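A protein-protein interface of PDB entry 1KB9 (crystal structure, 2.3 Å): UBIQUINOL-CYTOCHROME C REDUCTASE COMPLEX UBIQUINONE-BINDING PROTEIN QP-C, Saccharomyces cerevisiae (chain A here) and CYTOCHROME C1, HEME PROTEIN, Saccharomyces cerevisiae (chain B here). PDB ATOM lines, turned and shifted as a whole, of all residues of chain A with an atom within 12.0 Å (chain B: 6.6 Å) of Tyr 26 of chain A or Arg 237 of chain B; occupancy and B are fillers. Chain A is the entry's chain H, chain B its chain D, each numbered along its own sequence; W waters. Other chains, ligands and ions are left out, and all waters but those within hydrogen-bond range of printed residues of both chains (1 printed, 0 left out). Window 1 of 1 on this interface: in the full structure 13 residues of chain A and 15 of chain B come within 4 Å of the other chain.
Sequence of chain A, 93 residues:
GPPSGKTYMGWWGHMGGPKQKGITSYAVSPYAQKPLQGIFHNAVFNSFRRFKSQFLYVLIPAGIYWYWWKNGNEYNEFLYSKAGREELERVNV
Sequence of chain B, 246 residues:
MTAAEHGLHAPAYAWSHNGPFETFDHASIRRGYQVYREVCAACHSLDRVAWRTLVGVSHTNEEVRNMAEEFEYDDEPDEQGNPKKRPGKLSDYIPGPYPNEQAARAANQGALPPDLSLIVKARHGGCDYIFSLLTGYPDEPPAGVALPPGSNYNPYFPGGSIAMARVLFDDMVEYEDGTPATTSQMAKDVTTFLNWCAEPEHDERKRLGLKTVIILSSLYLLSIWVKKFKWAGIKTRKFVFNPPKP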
ATOM      1  N   TRP A  12      -5.045  -4.438  31.891  1.00  0.00           N
ATOM      2  CA  TRP A  12      -4.614  -3.911  30.596  1.00  0.00           C
ATOM      3  C   TRP A  12      -3.878  -2.580  30.723  1.00  0.00           C
ATOM      4  O   TRP A  12      -4.433  -1.596  31.233  1.00  0.00           O
ATOM      5  CB  TRP A  12      -5.820  -3.757  29.680  1.00  0.00           C
ATOM      6  CG  TRP A  12      -6.540  -5.045  29.474  1.00  0.00           C
ATOM      7  CD1 TRP A  12      -7.756  -5.386  29.969  1.00  0.00           C
ATOM      8  CD2 TRP A  12      -6.083  -6.168  28.711  1.00  0.00           C
ATOM      9  NE1 TRP A  12      -8.094  -6.652  29.564  1.00  0.00           N
ATOM     10  CE2 TRP A  12      -7.085  -7.156  28.787  1.00  0.00           C
ATOM     11  CE3 TRP A  12      -4.923  -6.434  27.967  1.00  0.00           C
ATOM     12  CZ2 TRP A  12      -6.970  -8.400  28.139  1.00  0.00           C
ATOM     13  CZ3 TRP A  12      -4.807  -7.669  27.322  1.00  0.00           C
ATOM     14  CH2 TRP A  12      -5.826  -8.634  27.412  1.00  0.00           C
ATOM     15  N   MET A  15      -0.122  -4.849  33.329  1.00  0.00           N
ATOM     16  CA  MET A  15      -0.272  -6.257  33.678  1.00  0.00           C
ATOM     17  C   MET A  15       0.688  -6.748  34.742  1.00  0.00           C
ATOM     18  O   MET A  15       0.388  -7.714  35.450  1.00  0.00           O
ATOM     19  CB  MET A  15      -0.156  -7.138  32.437  1.00  0.00           C
ATOM     20  CG  MET A  15      -0.984  -8.411  32.517  1.00  0.00           C
ATOM     21  SD  MET A  15      -2.754  -8.064  32.611  1.00  0.00           S
ATOM     22  CE  MET A  15      -3.106  -7.636  30.906  1.00  0.00           C
ATOM     23  N   GLN A  20       8.597  -4.919  27.629  1.00  0.00           N
ATOM     24  CA  GLN A  20       8.856  -5.602  26.367  1.00  0.00           C
ATOM     25  C   GLN A  20       9.390  -4.651  25.312  1.00  0.00           C
ATOM     26  O   GLN A  20       8.904  -3.533  25.171  1.00  0.00           O
ATOM     27  CB  GLN A  20       7.580  -6.274  25.848  1.00  0.00           C
ATOM     28  CG  GLN A  20       7.021  -7.355  26.757  1.00  0.00           C
ATOM     29  CD  GLN A  20       5.771  -7.994  26.186  1.00  0.00           C
ATOM     30  OE1 GLN A  20       5.571  -8.004  24.972  1.00  0.00           O
ATOM     31  NE2 GLN A  20       4.920  -8.529  27.057  1.00  0.00           N
ATOM     32  N   GLY A  22      11.513  -4.996  21.214  1.00  0.00           N
ATOM     33  CA  GLY A  22      12.113  -5.842  20.200  1.00  0.00           C
ATOM     34  C   GLY A  22      11.243  -6.935  19.613  1.00  0.00           C
ATOM     35  O   GLY A  22      11.586  -7.518  18.582  1.00  0.00           O
ATOM     36  N   ILE A  23      10.134  -7.243  20.279  1.00  0.00           N
ATOM     37  CA  ILE A  23       9.217  -8.281  19.806  1.00  0.00           C
ATOM     38  C   ILE A  23       8.128  -7.631  18.957  1.00  0.00           C
ATOM     39  O   ILE A  23       7.484  -6.677  19.388  1.00  0.00           O
ATOM     40  CB  ILE A  23       8.554  -9.008  20.993  1.00  0.00           C
ATOM     41  CG1 ILE A  23       9.630  -9.538  21.947  1.00  0.00           C
ATOM     42  CG2 ILE A  23       7.647 -10.129  20.486  1.00  0.00           C
ATOM     43  CD1 ILE A  23       9.110  -9.956  23.302  1.00  0.00           C
ATOM     44  N   THR A  24       7.928  -8.155  17.754  1.00  0.00           N
ATOM     45  CA  THR A  24       6.925  -7.647  16.833  1.00  0.00           C
ATOM     46  C   THR A  24       5.994  -8.802  16.479  1.00  0.00           C
ATOM     47  O   THR A  24       6.459  -9.884  16.126  1.00  0.00           O
ATOM     48  CB  THR A  24       7.607  -7.098  15.539  1.00  0.00           C
ATOM     49  OG1 THR A  24       8.437  -5.984  15.881  1.00  0.00           O
ATOM     50  CG2 THR A  24       6.583  -6.654  14.502  1.00  0.00           C
ATOM     51  N   SER A  25       4.683  -8.592  16.584  1.00  0.00           N
ATOM     52  CA  SER A  25       3.745  -9.662  16.263  1.00  0.00           C
ATOM     53  C   SER A  25       2.917  -9.344  15.040  1.00  0.00           C
ATOM     54  O   SER A  25       2.687  -8.181  14.718  1.00  0.00           O
ATOM     55  CB  SER A  25       2.832  -9.985  17.457  1.00  0.00           C
ATOM     56  OG  SER A  25       1.981  -8.901  17.788  1.00  0.00           O
ATOM     57  N   TYR A  26       2.472 -10.385  14.355  1.00  0.00           N
ATOM     58  CA  TYR A  26       1.669 -10.216  13.154  1.00  0.00           C
ATOM     59  C   TYR A  26       0.496 -11.169  13.220  1.00  0.00           C
ATOM     60  O   TYR A  26       0.627 -12.278  13.739  1.00  0.00           O
ATOM     61  CB  TYR A  26       2.485 -10.560  11.900  1.00  0.00           C
ATOM     62  CG  TYR A  26       3.754  -9.761  11.710  1.00  0.00           C
ATOM     63  CD1 TYR A  26       4.925 -10.105  12.387  1.00  0.00           C
ATOM     64  CD2 TYR A  26       3.802  -8.694  10.809  1.00  0.00           C
ATOM     65  CE1 TYR A  26       6.108  -9.412  12.169  1.00  0.00           C
ATOM     66  CE2 TYR A  26       4.986  -7.997  10.580  1.00  0.00           C
ATOM     67  CZ  TYR A  26       6.133  -8.361  11.260  1.00  0.00           C
ATOM     68  OH  TYR A  26       7.313  -7.690  11.024  1.00  0.00           O
ATOM     69  N   ALA A  27      -0.635 -10.755  12.659  1.00  0.00           N
ATOM     70  CA  ALA A  27      -1.815 -11.599  12.637  1.00  0.00           C
ATOM     71  C   ALA A  27      -2.680 -11.228  11.434  1.00  0.00           C
ATOM     72  O   ALA A  27      -2.565 -10.131  10.892  1.00  0.00           O
ATOM     73  CB  ALA A  27      -2.611 -11.457  13.950  1.00  0.00           C
ATOM     74  N   VAL A  28      -3.567 -12.139  11.054  1.00  0.00           N
ATOM     75  CA  VAL A  28      -4.442 -11.935   9.916  1.00  0.00           C
ATOM     76  C   VAL A  28      -5.883 -12.257  10.299  1.00  0.00           C
ATOM     77  O   VAL A  28      -6.156 -13.284  10.926  1.00  0.00           O
ATOM     78  CB  VAL A  28      -4.003 -12.834   8.723  1.00  0.00           C
ATOM     79  CG1 VAL A  28      -5.047 -12.809   7.621  1.00  0.00           C
ATOM     80  CG2 VAL A  28      -2.666 -12.350   8.173  1.00  0.00           C
ATOM     81  N   SER A  29      -6.800 -11.385   9.894  1.00  0.00           N
ATOM     82  CA  SER A  29      -8.211 -11.551  10.188  1.00  0.00           C
ATOM     83  C   SER A  29      -8.741 -12.940   9.870  1.00  0.00           C
ATOM     84  O   SER A  29      -8.392 -13.532   8.845  1.00  0.00           O
ATOM     85  CB  SER A  29      -9.041 -10.529   9.411  1.00  0.00           C
ATOM     86  OG  SER A  29     -10.432 -10.789   9.543  1.00  0.00           O
ATOM     87  N   PRO A  30      -9.547 -13.503  10.786  1.00  0.00           N
ATOM     88  CA  PRO A  30     -10.144 -14.826  10.610  1.00  0.00           C
ATOM     89  C   PRO A  30     -11.042 -14.796   9.377  1.00  0.00           C
ATOM     90  O   PRO A  30     -11.294 -15.825   8.758  1.00  0.00           O
ATOM     91  CB  PRO A  30     -10.976 -14.987  11.880  1.00  0.00           C
ATOM     92  CG  PRO A  30     -10.135 -14.284  12.900  1.00  0.00           C
ATOM     93  CD  PRO A  30      -9.740 -13.021  12.168  1.00  0.00           C
ATOM     94  N   ALA A  32     -10.389 -13.295   6.523  1.00  0.00           N
ATOM     95  CA  ALA A  32      -9.543 -13.465   5.350  1.00  0.00           C
ATOM     96  C   ALA A  32      -8.914 -14.851   5.262  1.00  0.00           C
ATOM     97  O   ALA A  32      -8.218 -15.160   4.292  1.00  0.00           O
ATOM     98  CB  ALA A  32      -8.449 -12.408   5.351  1.00  0.00           C
ATOM     99  N   GLN A  33      -9.142 -15.678   6.276  1.00  0.00           N
ATOM    100  CA  GLN A  33      -8.561 -17.013   6.300  1.00  0.00           C
ATOM    101  C   GLN A  33      -9.428 -18.080   5.666  1.00  0.00           C
ATOM    102  O   GLN A  33     -10.649 -17.952   5.577  1.00  0.00           O
ATOM    103  CB  GLN A  33      -8.177 -17.414   7.726  1.00  0.00           C
ATOM    104  CG  GLN A  33      -7.127 -16.509   8.349  1.00  0.00           C
ATOM    105  CD  GLN A  33      -6.671 -16.986   9.716  1.00  0.00           C
ATOM    106  OE1 GLN A  33      -6.634 -18.189   9.987  1.00  0.00           O
ATOM    107  NE2 GLN A  33      -6.305 -16.045  10.580  1.00  0.00           N
ATOM    108  N   ALA B 232      -8.985 -18.208  15.009  1.00  0.00           N
ATOM    109  CA  ALA B 232      -8.038 -18.239  13.877  1.00  0.00           C
ATOM    110  C   ALA B 232      -6.945 -17.168  13.882  1.00  0.00           C
ATOM    111  O   ALA B 232      -5.800 -17.449  13.540  1.00  0.00           O
ATOM    112  CB  ALA B 232      -8.781 -18.242  12.536  1.00  0.00           C
ATOM    113  N   GLY B 233      -7.283 -15.952  14.283  1.00  0.00           N
ATOM    114  CA  GLY B 233      -6.280 -14.907  14.328  1.00  0.00           C
ATOM    115  C   GLY B 233      -5.197 -15.174  15.362  1.00  0.00           C
ATOM    116  O   GLY B 233      -4.023 -14.879  15.128  1.00  0.00           O
ATOM    117  N   ILE B 234      -5.591 -15.736  16.505  1.00  0.00           N
ATOM    118  CA  ILE B 234      -4.659 -16.039  17.599  1.00  0.00           C
ATOM    119  C   ILE B 234      -3.813 -17.271  17.292  1.00  0.00           C
ATOM    120  O   ILE B 234      -2.597 -17.268  17.481  1.00  0.00           O
ATOM    121  CB  ILE B 234      -5.429 -16.236  18.952  1.00  0.00           C
ATOM    122  CG1 ILE B 234      -6.041 -14.909  19.401  1.00  0.00           C
ATOM    123  CG2 ILE B 234      -4.517 -16.785  20.039  1.00  0.00           C
ATOM    124  CD1 ILE B 234      -5.032 -13.807  19.633  1.00  0.00           C
ATOM    125  N   LYS B 235      -4.458 -18.305  16.769  1.00  0.00           N
ATOM    126  CA  LYS B 235      -3.779 -19.548  16.443  1.00  0.00           C
ATOM    127  C   LYS B 235      -2.690 -19.408  15.383  1.00  0.00           C
ATOM    128  O   LYS B 235      -1.633 -20.032  15.487  1.00  0.00           O
ATOM    129  CB  LYS B 235      -4.798 -20.597  16.005  1.00  0.00           C
ATOM    130  CG  LYS B 235      -5.705 -21.088  17.117  1.00  0.00           C
ATOM    131  CD  LYS B 235      -5.043 -22.187  17.929  1.00  0.00           C
ATOM    132  CE  LYS B 235      -6.026 -22.805  18.916  1.00  0.00           C
ATOM    133  NZ  LYS B 235      -5.497 -24.021  19.590  1.00  0.00           N
ATOM    134  N   THR B 236      -2.939 -18.587  14.370  1.00  0.00           N
ATOM    135  CA  THR B 236      -1.962 -18.412  13.305  1.00  0.00           C
ATOM    136  C   THR B 236      -1.058 -17.199  13.486  1.00  0.00           C
ATOM    137  O   THR B 236      -0.239 -16.897  12.630  1.00  0.00           O
ATOM    138  CB  THR B 236      -2.649 -18.373  11.936  1.00  0.00           C
ATOM    139  OG1 THR B 236      -3.627 -17.328  11.923  1.00  0.00           O
ATOM    140  CG2 THR B 236      -3.335 -19.712  11.660  1.00  0.00           C
ATOM    141  N   ARG B 237      -1.195 -16.531  14.621  1.00  0.00           N
ATOM    142  CA  ARG B 237      -0.400 -15.355  14.958  1.00  0.00           C
ATOM    143  C   ARG B 237       1.093 -15.717  14.900  1.00  0.00           C
ATOM    144  O   ARG B 237       1.465 -16.849  15.207  1.00  0.00           O
ATOM    145  CB  ARG B 237      -0.806 -14.901  16.367  1.00  0.00           C
ATOM    146  CG  ARG B 237      -0.123 -13.670  16.912  1.00  0.00           C
ATOM    147  CD  ARG B 237      -0.777 -13.260  18.235  1.00  0.00           C
ATOM    148  NE  ARG B 237      -0.826 -14.365  19.193  1.00  0.00           N
ATOM    149  CZ  ARG B 237      -0.902 -14.219  20.515  1.00  0.00           C
ATOM    150  NH1 ARG B 237      -0.928 -15.291  21.297  1.00  0.00           N
ATOM    151  NH2 ARG B 237      -0.964 -13.008  21.059  1.00  0.00           N
ATOM    152  N   LYS B 238       1.935 -14.777  14.471  1.00  0.00           N
ATOM    153  CA  LYS B 238       3.376 -15.025  14.372  1.00  0.00           C
ATOM    154  C   LYS B 238       4.222 -13.934  15.008  1.00  0.00           C
ATOM    155  O   LYS B 238       3.925 -12.748  14.877  1.00  0.00           O
ATOM    156  CB  LYS B 238       3.793 -15.225  12.909  1.00  0.00           C
ATOM    157  CG  LYS B 238       3.050 -16.371  12.241  1.00  0.00           C
ATOM    158  CD  LYS B 238       3.689 -16.848  10.959  1.00  0.00           C
ATOM    159  CE  LYS B 238       2.901 -18.027  10.401  1.00  0.00           C
ATOM    160  NZ  LYS B 238       3.542 -18.643   9.200  1.00  0.00           N
ATOM    161  N   PHE B 239       5.280 -14.345  15.699  1.00  0.00           N
ATOM    162  CA  PHE B 239       6.183 -13.408  16.369  1.00  0.00           C
ATOM    163  C   PHE B 239       7.598 -13.370  15.752  1.00  0.00           C
ATOM    164  O   PHE B 239       8.050 -14.337  15.128  1.00  0.00           O
ATOM    165  CB  PHE B 239       6.304 -13.766  17.859  1.00  0.00           C
ATOM    166  CG  PHE B 239       5.039 -13.558  18.651  1.00  0.00           C
ATOM    167  CD1 PHE B 239       4.034 -14.524  18.656  1.00  0.00           C
ATOM    168  CD2 PHE B 239       4.853 -12.398  19.395  1.00  0.00           C
ATOM    169  CE1 PHE B 239       2.858 -14.338  19.392  1.00  0.00           C
ATOM    170  CE2 PHE B 239       3.682 -12.200  20.134  1.00  0.00           C
ATOM    171  CZ  PHE B 239       2.684 -13.176  20.128  1.00  0.00           C
ATOM    172  N   VAL B 240       8.269 -12.227  15.900  1.00  0.00           N
ATOM    173  CA  VAL B 240       9.645 -12.048  15.431  1.00  0.00           C
ATOM    174  C   VAL B 240      10.394 -11.226  16.479  1.00  0.00           C
ATOM    175  O   VAL B 240       9.878 -10.244  17.002  1.00  0.00           O
ATOM    176  CB  VAL B 240       9.754 -11.330  14.059  1.00  0.00           C
ATOM    177  CG1 VAL B 240       9.061 -12.124  12.982  1.00  0.00           C
ATOM    178  CG2 VAL B 240       9.201  -9.924  14.138  1.00  0.00           C
ATOM    179  N   ASN B 242      13.857  -9.031  17.399  1.00  0.00           N
ATOM    180  CA  ASN B 242      15.023  -8.303  16.927  1.00  0.00           C
ATOM    181  C   ASN B 242      15.613  -7.681  18.186  1.00  0.00           C
ATOM    182  O   ASN B 242      15.122  -6.662  18.672  1.00  0.00           O
ATOM    183  CB  ASN B 242      14.628  -7.217  15.918  1.00  0.00           C
ATOM    184  CG  ASN B 242      14.249  -7.789  14.569  1.00  0.00           C
ATOM    185  OD1 ASN B 242      14.944  -8.646  14.035  1.00  0.00           O
ATOM    186  ND2 ASN B 242      13.144  -7.321  14.012  1.00  0.00           N
HETATM  187  O   HOH W   1      -3.119 -14.477  12.441  1.00  0.00           O
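N of Thr 24 of chain A lies within hydrogen-bond range of O of Val 240 of chain B (3.0 Å). The backbone carbonyl oxygen of Lys 238 of chain B lies within hydrogen-bond range of the backbone NH of Tyr 26 of chain A, at 2.8 Å. The backbone carbonyl oxygen of Ala 232 of chain B is in hydrogen-bond range of the side-chain amide nitrogen of Gln 33 of chain A (3.3 Å). The backbone NH (N) of Asn 242 of chain B sits at hydrogen-bond distance from the backbone carbonyl oxygen (O) of Gly 22 of chain A, 3.0 Å away. The side-chain amide nitrogen (NE2) of Gln 33 of chain A sits at hydrogen-bond distance from the side-chain hydroxyl (OG1) of Thr 236 of chain B.
Gly 22 of chain A touches Val 240 of chain B (O to O, 3.6 Å). Ser 25 of chain A touches Lys 238 of chain B (CA to O, 3.4 Å). Phe 239 of chain B touches Ser 25 of chain A. Arg 237 of chain B touches Tyr 26 of chain A (CA to O, 3.5 Å). Val 240 of chain B touches Tyr 26 of chain A. Gly 233 of chain B touches Ala 27 of chain A. O of Val 28 of chain A touches CA of Gly 233 of chain B, 3.8 Å away. Pro 30 of chain A touches Ala 232 of chain B. Pro 30 of chain A touches Gly 233 of chain B (CG to N, 3.6 Å). Gly 233 of chain B touches Gln 33 of chain A (N to NE2, 3.8 Å).
The backbone carbonyl oxygen (O) of Ala 232 of chain B sits at hydrogen-bond distance from the side-chain hydroxyl (OG1) of Thr 236 of chain B (2.7 Å). The backbone carbonyl oxygen (O) of Val 28 of chain A lies within hydrogen-bond range of the side-chain amide nitrogen (NE2) of Gln 33 of chain A, at 2.8 Å.
Of the printed residues of chain B, Ile 23 of chain A touches Phe 239 (3.8 Å) and Val 240 (3.5 Å). Of the printed residues of chain B, Tyr 26 of chain A touches Arg 237 (3.5 Å), Lys 238 (2.8 Å) and Val 240 (3.7 Å). Of the printed residues of chain B, Ala 27 of chain A touches Gly 233. Of the printed residues of chain B, Pro 30 of chain A touches Ala 232 and Gly 233. Of the printed residues of chain B, Gln 33 of chain A touches Ala 232 (3.3 Å), Gly 233 (3.8 Å) and Thr 236 (3.3 Å). Of chain A, only Ala 27 (3.9 Å), Val 28 (3.8 Å), Pro 30 (3.6 Å) and Gln 33 (3.8 Å) come within 4 Å of Gly 233 of chain B. No residue of chain A comes within 4 Å of Ile 234 of chain B. Of the printed residues of chain A, Arg 237 of chain B touches Tyr 26 (3.5 Å). Of the printed residues of chain A, Lys 238 of chain B touches Ser 25 and Tyr 26. Phe 239 of chain B touches just these residues of chain A: Ile 23 (3.8 Å), Thr 24 (3.5 Å) and Ser 25 (3.6 Å). Val 240 of chain B touches four residues of chain A. Printed residues of chain A within 4 Å of Asn 242 of chain B: Gly 22 (3.0 Å). The nearest residue of chain B that does not touch Tyr 26 of chain A is Thr 236 of chain B (4.8 Å).
Hydrophobic or aromatic side chains of chain B within 4 Å of the printed part of chain A: Ala 232, Phe 239 and Val 240. Printed residues of chain A that touch a printed residue of chain B: Gly 22, Ile 23, Thr 24, Ser 25, Tyr 26, Ala 27, Val 28, Pro 30 and Gln 33. Hydrophobic or aromatic side chains of chain A within 4 Å of the printed part of chain B: Ile 23, Tyr 26, Ala 27 and Pro 30.
Water W1 lies within hydrogen-bond range of the backbone NH (N) of Val 28 of chain A (2.8 Å), the backbone carbonyl oxygen (O) of Gly 233 of chain B (2.9 Å) and the side-chain hydroxyl (OG1) of Thr 236 of chain B (2.9 Å).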
